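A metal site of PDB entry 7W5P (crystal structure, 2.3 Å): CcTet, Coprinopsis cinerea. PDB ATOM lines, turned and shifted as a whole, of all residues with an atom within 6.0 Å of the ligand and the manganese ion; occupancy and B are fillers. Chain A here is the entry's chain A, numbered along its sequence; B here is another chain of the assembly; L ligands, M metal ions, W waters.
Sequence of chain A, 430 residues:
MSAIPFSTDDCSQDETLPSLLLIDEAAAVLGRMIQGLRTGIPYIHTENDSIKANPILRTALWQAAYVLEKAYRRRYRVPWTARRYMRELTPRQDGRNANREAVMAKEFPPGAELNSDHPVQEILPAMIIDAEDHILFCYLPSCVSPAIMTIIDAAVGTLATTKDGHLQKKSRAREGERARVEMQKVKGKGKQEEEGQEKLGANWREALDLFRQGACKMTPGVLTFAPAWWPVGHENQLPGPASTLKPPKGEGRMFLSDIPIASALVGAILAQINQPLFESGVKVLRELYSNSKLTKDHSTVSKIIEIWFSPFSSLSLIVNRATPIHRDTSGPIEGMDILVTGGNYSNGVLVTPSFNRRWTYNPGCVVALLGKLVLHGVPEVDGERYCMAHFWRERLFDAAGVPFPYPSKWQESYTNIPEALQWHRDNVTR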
ATOM      1  N   TRP A 204     -17.984  28.143  15.451  1.00  0.00           N
ATOM      2  CA  TRP A 204     -18.580  27.626  14.197  1.00  0.00           C
ATOM      3  C   TRP A 204     -20.013  28.131  13.960  1.00  0.00           C
ATOM      4  O   TRP A 204     -20.358  28.249  12.902  1.00  0.00           O
ATOM      5  CB  TRP A 204     -18.421  26.107  14.070  1.00  0.00           C
ATOM      6  CG  TRP A 204     -19.253  25.281  14.986  1.00  0.00           C
ATOM      7  CD1 TRP A 204     -18.842  24.668  16.117  1.00  0.00           C
ATOM      8  CD2 TRP A 204     -20.644  25.004  14.887  1.00  0.00           C
ATOM      9  NE1 TRP A 204     -19.859  24.017  16.717  1.00  0.00           N
ATOM     10  CE2 TRP A 204     -20.978  24.183  15.978  1.00  0.00           C
ATOM     11  CE3 TRP A 204     -21.622  25.319  13.983  1.00  0.00           C
ATOM     12  CZ2 TRP A 204     -22.250  23.668  16.184  1.00  0.00           C
ATOM     13  CZ3 TRP A 204     -22.871  24.852  14.201  1.00  0.00           C
ATOM     14  CH2 TRP A 204     -23.177  24.026  15.269  1.00  0.00           C
ATOM     15  N   ARG A 205     -20.760  28.411  14.992  1.00  0.00           N
ATOM     16  CA  ARG A 205     -22.148  28.904  14.861  1.00  0.00           C
ATOM     17  C   ARG A 205     -22.206  30.261  14.170  1.00  0.00           C
ATOM     18  O   ARG A 205     -23.177  30.594  13.649  1.00  0.00           O
ATOM     19  CB  ARG A 205     -22.829  28.907  16.233  1.00  0.00           C
ATOM     20  CG  ARG A 205     -22.946  27.538  16.843  1.00  0.00           C
ATOM     21  CD  ARG A 205     -23.579  27.733  18.152  1.00  0.00           C
ATOM     22  NE  ARG A 205     -23.706  26.550  18.901  1.00  0.00           N
ATOM     23  CZ  ARG A 205     -24.543  25.565  18.795  1.00  0.00           C
ATOM     24  NH1 ARG A 205     -25.468  25.536  17.890  1.00  0.00           N
ATOM     25  NH2 ARG A 205     -24.464  24.611  19.640  1.00  0.00           N
ATOM     26  N   ILE A 318     -31.283  31.398  13.972  1.00  0.00           N
ATOM     27  CA  ILE A 318     -30.163  31.290  13.051  1.00  0.00           C
ATOM     28  C   ILE A 318     -30.682  31.661  11.659  1.00  0.00           C
ATOM     29  O   ILE A 318     -31.454  30.910  11.058  1.00  0.00           O
ATOM     30  CB  ILE A 318     -29.551  29.890  13.071  1.00  0.00           C
ATOM     31  CG1 ILE A 318     -29.147  29.508  14.496  1.00  0.00           C
ATOM     32  CG2 ILE A 318     -28.360  29.799  12.141  1.00  0.00           C
ATOM     33  CD1 ILE A 318     -30.131  28.586  15.193  1.00  0.00           C
ATOM     34  N   ARG A 321     -27.942  30.559   7.566  1.00  0.00           N
ATOM     35  CA  ARG A 321     -26.713  29.836   7.868  1.00  0.00           C
ATOM     36  C   ARG A 321     -26.947  28.347   7.665  1.00  0.00           C
ATOM     37  O   ARG A 321     -27.888  27.786   8.234  1.00  0.00           O
ATOM     38  CB  ARG A 321     -26.242  30.123   9.306  1.00  0.00           C
ATOM     39  CG  ARG A 321     -24.797  29.735   9.576  1.00  0.00           C
ATOM     40  CD  ARG A 321     -24.572  29.351  11.034  1.00  0.00           C
ATOM     41  NE  ARG A 321     -25.226  28.088  11.384  1.00  0.00           N
ATOM     42  CZ  ARG A 321     -25.579  27.741  12.615  1.00  0.00           C
ATOM     43  NH1 ARG A 321     -25.350  28.571  13.638  1.00  0.00           N
ATOM     44  NH2 ARG A 321     -26.174  26.574  12.837  1.00  0.00           N
ATOM     45  N   ALA A 322     -26.118  27.726   6.844  1.00  0.00           N
ATOM     46  CA  ALA A 322     -26.023  26.280   6.813  1.00  0.00           C
ATOM     47  C   ALA A 322     -25.488  25.774   8.144  1.00  0.00           C
ATOM     48  O   ALA A 322     -24.843  26.509   8.906  1.00  0.00           O
ATOM     49  CB  ALA A 322     -25.139  25.819   5.661  1.00  0.00           C
ATOM     50  N   THR A 323     -25.730  24.495   8.434  1.00  0.00           N
ATOM     51  CA  THR A 323     -25.366  23.919   9.723  1.00  0.00           C
ATOM     52  C   THR A 323     -24.583  22.633   9.487  1.00  0.00           C
ATOM     53  O   THR A 323     -25.132  21.669   8.912  1.00  0.00           O
ATOM     54  CB  THR A 323     -26.621  23.656  10.564  1.00  0.00           C
ATOM     55  OG1 THR A 323     -27.272  24.895  10.843  1.00  0.00           O
ATOM     56  CG2 THR A 323     -26.247  22.982  11.864  1.00  0.00           C
ATOM     57  N   HIS A 326     -23.038  18.081  13.723  1.00  0.00           N
ATOM     58  CA  HIS A 326     -22.555  18.391  15.062  1.00  0.00           C
ATOM     59  C   HIS A 326     -23.480  17.754  16.082  1.00  0.00           C
ATOM     60  O   HIS A 326     -24.627  17.395  15.772  1.00  0.00           O
ATOM     61  CB  HIS A 326     -22.497  19.903  15.276  1.00  0.00           C
ATOM     62  CG  HIS A 326     -23.848  20.533  15.453  1.00  0.00           C
ATOM     63  ND1 HIS A 326     -24.728  20.711  14.403  1.00  0.00           N
ATOM     64  CD2 HIS A 326     -24.490  20.979  16.557  1.00  0.00           C
ATOM     65  CE1 HIS A 326     -25.838  21.255  14.852  1.00  0.00           C
ATOM     66  NE2 HIS A 326     -25.722  21.430  16.152  1.00  0.00           N
ATOM     67  N   ARG A 327     -22.999  17.661  17.313  1.00  0.00           N
ATOM     68  CA  ARG A 327     -23.817  17.441  18.486  1.00  0.00           C
ATOM     69  C   ARG A 327     -23.760  18.696  19.342  1.00  0.00           C
ATOM     70  O   ARG A 327     -22.687  19.307  19.466  1.00  0.00           O
ATOM     71  CB  ARG A 327     -23.339  16.234  19.315  1.00  0.00           C
ATOM     72  CG  ARG A 327     -23.712  14.852  18.790  1.00  0.00           C
ATOM     73  CD  ARG A 327     -23.234  13.773  19.777  1.00  0.00           C
ATOM     74  NE  ARG A 327     -23.127  12.433  19.178  1.00  0.00           N
ATOM     75  CZ  ARG A 327     -22.032  11.951  18.613  1.00  0.00           C
ATOM     76  NH1 ARG A 327     -20.924  12.698  18.559  1.00  0.00           N
ATOM     77  NH2 ARG A 327     -22.029  10.722  18.103  1.00  0.00           N
ATOM     78  N   ASP A 328     -24.902  19.091  19.898  1.00  0.00           N
ATOM     79  CA  ASP A 328     -24.920  20.199  20.858  1.00  0.00           C
ATOM     80  C   ASP A 328     -24.529  19.635  22.220  1.00  0.00           C
ATOM     81  O   ASP A 328     -25.242  18.803  22.788  1.00  0.00           O
ATOM     82  CB  ASP A 328     -26.299  20.857  20.892  1.00  0.00           C
ATOM     83  CG  ASP A 328     -26.765  21.317  19.522  1.00  0.00           C
ATOM     84  OD1 ASP A 328     -26.167  22.268  18.958  1.00  0.00           O
ATOM     85  OD2 ASP A 328     -27.752  20.729  19.006  1.00  0.00           O
ATOM     86  N   LEU A 339     -36.274  21.971  16.772  1.00  0.00           N
ATOM     87  CA  LEU A 339     -35.894  22.832  15.658  1.00  0.00           C
ATOM     88  C   LEU A 339     -37.117  23.104  14.796  1.00  0.00           C
ATOM     89  O   LEU A 339     -37.886  22.195  14.487  1.00  0.00           O
ATOM     90  CB  LEU A 339     -34.810  22.185  14.807  1.00  0.00           C
ATOM     91  CG  LEU A 339     -33.579  21.664  15.533  1.00  0.00           C
ATOM     92  CD1 LEU A 339     -32.765  20.793  14.596  1.00  0.00           C
ATOM     93  CD2 LEU A 339     -32.762  22.850  16.049  1.00  0.00           C
ATOM     94  N   VAL A 340     -37.283  24.373  14.422  1.00  0.00           N
ATOM     95  CA  VAL A 340     -38.318  24.808  13.481  1.00  0.00           C
ATOM     96  C   VAL A 340     -37.604  25.563  12.371  1.00  0.00           C
ATOM     97  O   VAL A 340     -36.860  26.507  12.639  1.00  0.00           O
ATOM     98  CB  VAL A 340     -39.377  25.701  14.149  1.00  0.00           C
ATOM     99  CG1 VAL A 340     -40.486  26.046  13.173  1.00  0.00           C
ATOM    100  CG2 VAL A 340     -39.944  25.023  15.402  1.00  0.00           C
ATOM    101  N   THR A 341     -37.798  25.138  11.128  1.00  0.00           N
ATOM    102  CA  THR A 341     -37.152  25.787   9.999  1.00  0.00           C
ATOM    103  C   THR A 341     -38.191  26.488   9.125  1.00  0.00           C
ATOM    104  O   THR A 341     -39.334  26.041   9.006  1.00  0.00           O
ATOM    105  CB  THR A 341     -36.341  24.779   9.175  1.00  0.00           C
ATOM    106  OG1 THR A 341     -35.625  25.464   8.132  1.00  0.00           O
ATOM    107  CG2 THR A 341     -37.227  23.709   8.565  1.00  0.00           C
ATOM    108  N   LEU A 350     -32.062  17.634   6.373  1.00  0.00           N
ATOM    109  CA  LEU A 350     -31.417  17.444   7.668  1.00  0.00           C
ATOM    110  C   LEU A 350     -30.790  16.061   7.686  1.00  0.00           C
ATOM    111  O   LEU A 350     -31.450  15.070   7.379  1.00  0.00           O
ATOM    112  CB  LEU A 350     -32.408  17.619   8.825  1.00  0.00           C
ATOM    113  CG  LEU A 350     -31.775  17.567  10.228  1.00  0.00           C
ATOM    114  CD1 LEU A 350     -32.187  18.763  11.073  1.00  0.00           C
ATOM    115  CD2 LEU A 350     -32.139  16.277  10.936  1.00  0.00           C
ATOM    116  N   TYR A 361     -36.352  18.711   4.819  1.00  0.00           N
ATOM    117  CA  TYR A 361     -36.313  19.737   5.866  1.00  0.00           C
ATOM    118  C   TYR A 361     -36.715  21.082   5.259  1.00  0.00           C
ATOM    119  O   TYR A 361     -35.895  22.008   5.172  1.00  0.00           O
ATOM    120  CB  TYR A 361     -34.917  19.777   6.496  1.00  0.00           C
ATOM    121  CG  TYR A 361     -34.802  20.512   7.799  1.00  0.00           C
ATOM    122  CD1 TYR A 361     -35.535  20.131   8.926  1.00  0.00           C
ATOM    123  CD2 TYR A 361     -33.920  21.589   7.939  1.00  0.00           C
ATOM    124  CE1 TYR A 361     -35.412  20.799  10.122  1.00  0.00           C
ATOM    125  CE2 TYR A 361     -33.797  22.260   9.126  1.00  0.00           C
ATOM    126  CZ  TYR A 361     -34.543  21.867  10.213  1.00  0.00           C
ATOM    127  OH  TYR A 361     -34.405  22.547  11.415  1.00  0.00           O
ATOM    128  N   GLY A 371     -30.344  16.530  21.221  1.00  0.00           N
ATOM    129  CA  GLY A 371     -29.259  17.234  20.551  1.00  0.00           C
ATOM    130  C   GLY A 371     -27.879  16.825  21.039  1.00  0.00           C
ATOM    131  O   GLY A 371     -26.905  16.928  20.295  1.00  0.00           O
ATOM    132  N   HIS A 376     -26.400  15.943  13.754  1.00  0.00           N
ATOM    133  CA  HIS A 376     -27.321  16.542  12.807  1.00  0.00           C
ATOM    134  C   HIS A 376     -26.672  17.747  12.143  1.00  0.00           C
ATOM    135  O   HIS A 376     -25.875  18.454  12.769  1.00  0.00           O
ATOM    136  CB  HIS A 376     -28.636  16.954  13.470  1.00  0.00           C
ATOM    137  CG  HIS A 376     -28.461  17.928  14.590  1.00  0.00           C
ATOM    138  ND1 HIS A 376     -27.935  17.573  15.813  1.00  0.00           N
ATOM    139  CD2 HIS A 376     -28.776  19.244  14.680  1.00  0.00           C
ATOM    140  CE1 HIS A 376     -27.920  18.630  16.609  1.00  0.00           C
ATOM    141  NE2 HIS A 376     -28.420  19.659  15.951  1.00  0.00           N
ATOM    142  N   VAL A 378     -27.411  20.672   8.507  1.00  0.00           N
ATOM    143  CA  VAL A 378     -28.305  21.162   7.456  1.00  0.00           C
ATOM    144  C   VAL A 378     -27.482  21.839   6.372  1.00  0.00           C
ATOM    145  O   VAL A 378     -26.894  22.912   6.624  1.00  0.00           O
ATOM    146  CB  VAL A 378     -29.364  22.121   8.033  1.00  0.00           C
ATOM    147  CG1 VAL A 378     -30.277  22.617   6.918  1.00  0.00           C
ATOM    148  CG2 VAL A 378     -30.167  21.444   9.129  1.00  0.00           C
ATOM    149  N   ARG A 385     -33.329  31.072   4.453  1.00  0.00           N
ATOM    150  CA  ARG A 385     -33.807  30.160   5.483  1.00  0.00           C
ATOM    151  C   ARG A 385     -33.462  30.730   6.857  1.00  0.00           C
ATOM    152  O   ARG A 385     -32.470  31.439   7.010  1.00  0.00           O
ATOM    153  CB  ARG A 385     -33.181  28.760   5.317  1.00  0.00           C
ATOM    154  CG  ARG A 385     -33.504  27.766   6.428  1.00  0.00           C
ATOM    155  CD  ARG A 385     -32.900  26.396   6.131  1.00  0.00           C
ATOM    156  NE  ARG A 385     -31.591  26.238   6.742  1.00  0.00           N
ATOM    157  CZ  ARG A 385     -31.402  25.811   7.990  1.00  0.00           C
ATOM    158  NH1 ARG A 385     -32.444  25.503   8.745  1.00  0.00           N
ATOM    159  NH2 ARG A 385     -30.179  25.688   8.479  1.00  0.00           N
ATOM    160  N   TYR A 386     -34.319  30.434   7.827  1.00  0.00           N
ATOM    161  CA  TYR A 386     -34.061  30.684   9.225  1.00  0.00           C
ATOM    162  C   TYR A 386     -34.448  29.446  10.044  1.00  0.00           C
ATOM    163  O   TYR A 386     -35.258  28.621   9.606  1.00  0.00           O
ATOM    164  CB  TYR A 386     -34.814  31.920   9.738  1.00  0.00           C
ATOM    165  CG  TYR A 386     -36.315  31.768   9.712  1.00  0.00           C
ATOM    166  CD1 TYR A 386     -37.051  32.107   8.590  1.00  0.00           C
ATOM    167  CD2 TYR A 386     -36.996  31.270  10.821  1.00  0.00           C
ATOM    168  CE1 TYR A 386     -38.424  31.966   8.566  1.00  0.00           C
ATOM    169  CE2 TYR A 386     -38.363  31.131  10.809  1.00  0.00           C
ATOM    170  CZ  TYR A 386     -39.076  31.479   9.681  1.00  0.00           C
ATOM    171  OH  TYR A 386     -40.450  31.338   9.657  1.00  0.00           O
ATOM    172  N   CYS A 387     -33.846  29.332  11.228  1.00  0.00           N
ATOM    173  CA  CYS A 387     -34.102  28.220  12.135  1.00  0.00           C
ATOM    174  C   CYS A 387     -34.292  28.751  13.547  1.00  0.00           C
ATOM    175  O   CYS A 387     -33.523  29.603  13.995  1.00  0.00           O
ATOM    176  CB  CYS A 387     -32.968  27.185  12.089  1.00  0.00           C
ATOM    177  SG  CYS A 387     -32.969  26.007  13.476  1.00  0.00           S
ATOM    178  N   ALA A 389     -34.173  27.271  17.249  1.00  0.00           N
ATOM    179  CA  ALA A 389     -33.704  26.136  18.023  1.00  0.00           C
ATOM    180  C   ALA A 389     -34.072  26.375  19.489  1.00  0.00           C
ATOM    181  O   ALA A 389     -33.608  27.347  20.084  1.00  0.00           O
ATOM    182  CB  ALA A 389     -32.198  25.949  17.871  1.00  0.00           C
ATOM    183  P   6MA B   6     -22.281  27.194  24.715  1.00  0.00           P
ATOM    184  OP1 6MA B   6     -22.882  27.061  26.040  1.00  0.00           O
ATOM    185  OP2 6MA B   6     -22.209  26.220  23.599  1.00  0.00           O
ATOM    186  O5' 6MA B   6     -22.902  28.483  24.025  1.00  0.00           O
ATOM    187  C5' 6MA B   6     -22.309  29.147  22.834  1.00  0.00           C
ATOM    188  C4' 6MA B   6     -23.474  29.675  22.071  1.00  0.00           C
ATOM    189  O4' 6MA B   6     -24.049  28.565  21.427  1.00  0.00           O
ATOM    190  C3' 6MA B   6     -24.545  30.374  22.825  1.00  0.00           C
ATOM    191  O3' 6MA B   6     -24.985  31.623  22.360  1.00  0.00           O
ATOM    192  C2' 6MA B   6     -25.705  29.390  22.823  1.00  0.00           C
ATOM    193  C1' 6MA B   6     -25.479  28.560  21.584  1.00  0.00           C
ATOM    194  N9  6MA B   6     -26.050  27.294  21.783  1.00  0.00           N
ATOM    195  C8  6MA B   6     -25.762  26.443  22.831  1.00  0.00           C
ATOM    196  N7  6MA B   6     -26.438  25.310  22.799  1.00  0.00           N
ATOM    197  C5  6MA B   6     -27.227  25.416  21.644  1.00  0.00           C
ATOM    198  C6  6MA B   6     -28.129  24.503  21.116  1.00  0.00           C
ATOM    199  N1  6MA B   6     -28.773  24.926  19.906  1.00  0.00           N
ATOM    200  C2  6MA B   6     -28.448  26.151  19.408  1.00  0.00           C
ATOM    201  N3  6MA B   6     -27.569  27.011  19.933  1.00  0.00           N
ATOM    202  C4  6MA B   6     -26.997  26.619  21.031  1.00  0.00           C
ATOM    203  N6  6MA B   6     -28.463  23.273  21.644  1.00  0.00           N
ATOM    204  C1  6MA B   6     -29.605  22.706  20.941  1.00  0.00           C
HETATM  205  C1  LIG L   1     -27.912  24.271  15.478  1.00  0.00           C
HETATM  206  C2  LIG L   1     -28.895  23.405  14.669  1.00  0.00           C
HETATM  207  C3  LIG L   1     -30.437  23.262  12.705  1.00  0.00           C
HETATM  208  C4  LIG L   1     -30.768  24.141  11.480  1.00  0.00           C
HETATM  209  O1  LIG L   1     -27.356  23.815  16.513  1.00  0.00           O
HETATM  210  O2  LIG L   1     -27.686  25.449  15.107  1.00  0.00           O
HETATM  211  O3  LIG L   1     -29.127  22.256  15.064  1.00  0.00           O
HETATM  212  O4  LIG L   1     -31.876  23.960  10.935  1.00  0.00           O
HETATM  213  N1  LIG L   1     -29.472  23.965  13.581  1.00  0.00           N
HETATM  214  O5  LIG L   1     -29.901  24.969  11.130  1.00  0.00           O
HETATM  215 MN    MN M   1     -27.803  21.711  16.864  1.00  0.00          MN
HETATM  216  O   HOH W   1     -26.210  27.746  16.107  1.00  0.00           O
HETATM  217  O   HOH W   2     -29.495  22.694  17.735  1.00  0.00           O
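Water W1 lies within hydrogen-bond range of the guanidinium group (NH1) of Arg 321 (2.7 Å), an oxygen (O2) of the ligand (2.9 Å) and the guanidinium group (NH1) of Arg 205 (2.9 Å).
Ile 318 touches the ligand. Leu 339 touches the ligand. Val 378 touches the ligand (CG2 to O4, 3.5 Å). 6MA 6 of chain B touches the ligand. Hydrophobic or aromatic side chains that line the ligand: Ile 318, His 326, Leu 339, Tyr 361, His 376 and Val 378. Within 4 Å of the ligand: Arg 205, Ile 318, Arg 321, Thr 323, His 326, Asp 328, Leu 339, Tyr 361, His 376, Val 378, Arg 385, Cys 387 and 6MA 6 of chain B.
The side-chain hydroxyl (OH) of Tyr 361 sits at hydrogen-bond distance from an oxygen (O4) of the ligand (2.9 Å). The side-chain hydroxyl (OG1) of Thr 323 sits at hydrogen-bond distance from an oxygen (O5) of the ligand. An oxygen (O4) of the ligand is in hydrogen-bond range of the side-chain sulfur of Cys 387 (3.4 Å). An oxygen (O2) of the ligand lies within salt-bridge range of the guanidinium group of Arg 205. The guanidinium group of Arg 385 lies within salt-bridge range of an oxygen (O4) of the ligand, at 2.7 Å. The guanidinium group (NH2) of Arg 321 is in salt-bridge range of an oxygen (O2) of the ligand, at 3.0 Å.
The manganese ion is bound by water W2, an oxygen (O1) of the ligand, a ring nitrogen (NE2) of His 326, an oxygen (O3) of the ligand, a ring nitrogen (NE2) of His 376 and the side-chain carboxylate (OD2) of Asp 328. The manganese ion has six donor atoms within binding distance. Slightly farther from the manganese ion lies OD1 of Asp 328 (2.7 Å).
Within 4 Å of the manganese ion: His 326, Asp 328 and His 376. The nearest printed residue that does not touch the manganese ion is 6MA 6 of chain B (4.5 Å).
The backbone carbonyl oxygen of Ile 318 is in hydrogen-bond range of the backbone NH of Cys 387, 2.9 Å away. The side-chain hydroxyl (OG1) of Thr 323 is in hydrogen-bond range of the guanidinium group (NH2) of Arg 321 (2.8 Å). N of Asp 328 lies within hydrogen-bond range of O of Gly 371 (3.0 Å). The side-chain carboxylate (OD1) of Asp 328 lies within salt-bridge range of the guanidinium group (NH2) of Arg 205 (3.0 Å). The guanidinium group of Arg 385 sits at hydrogen-bond distance from the backbone carbonyl oxygen of Arg 321, at 3.1 Å. O4' of 6MA 6 of chain B sits at hydrogen-bond distance from NE of Arg 205, at 3.2 Å. The backbone NH (N) of Val 378 is in hydrogen-bond range of the backbone carbonyl oxygen (O) of Thr 323 (2.5 Å). The backbone carbonyl oxygen (O) of Arg 205 is in hydrogen-bond range of the guanidinium group (NH1) of Arg 321, 3.0 Å away.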
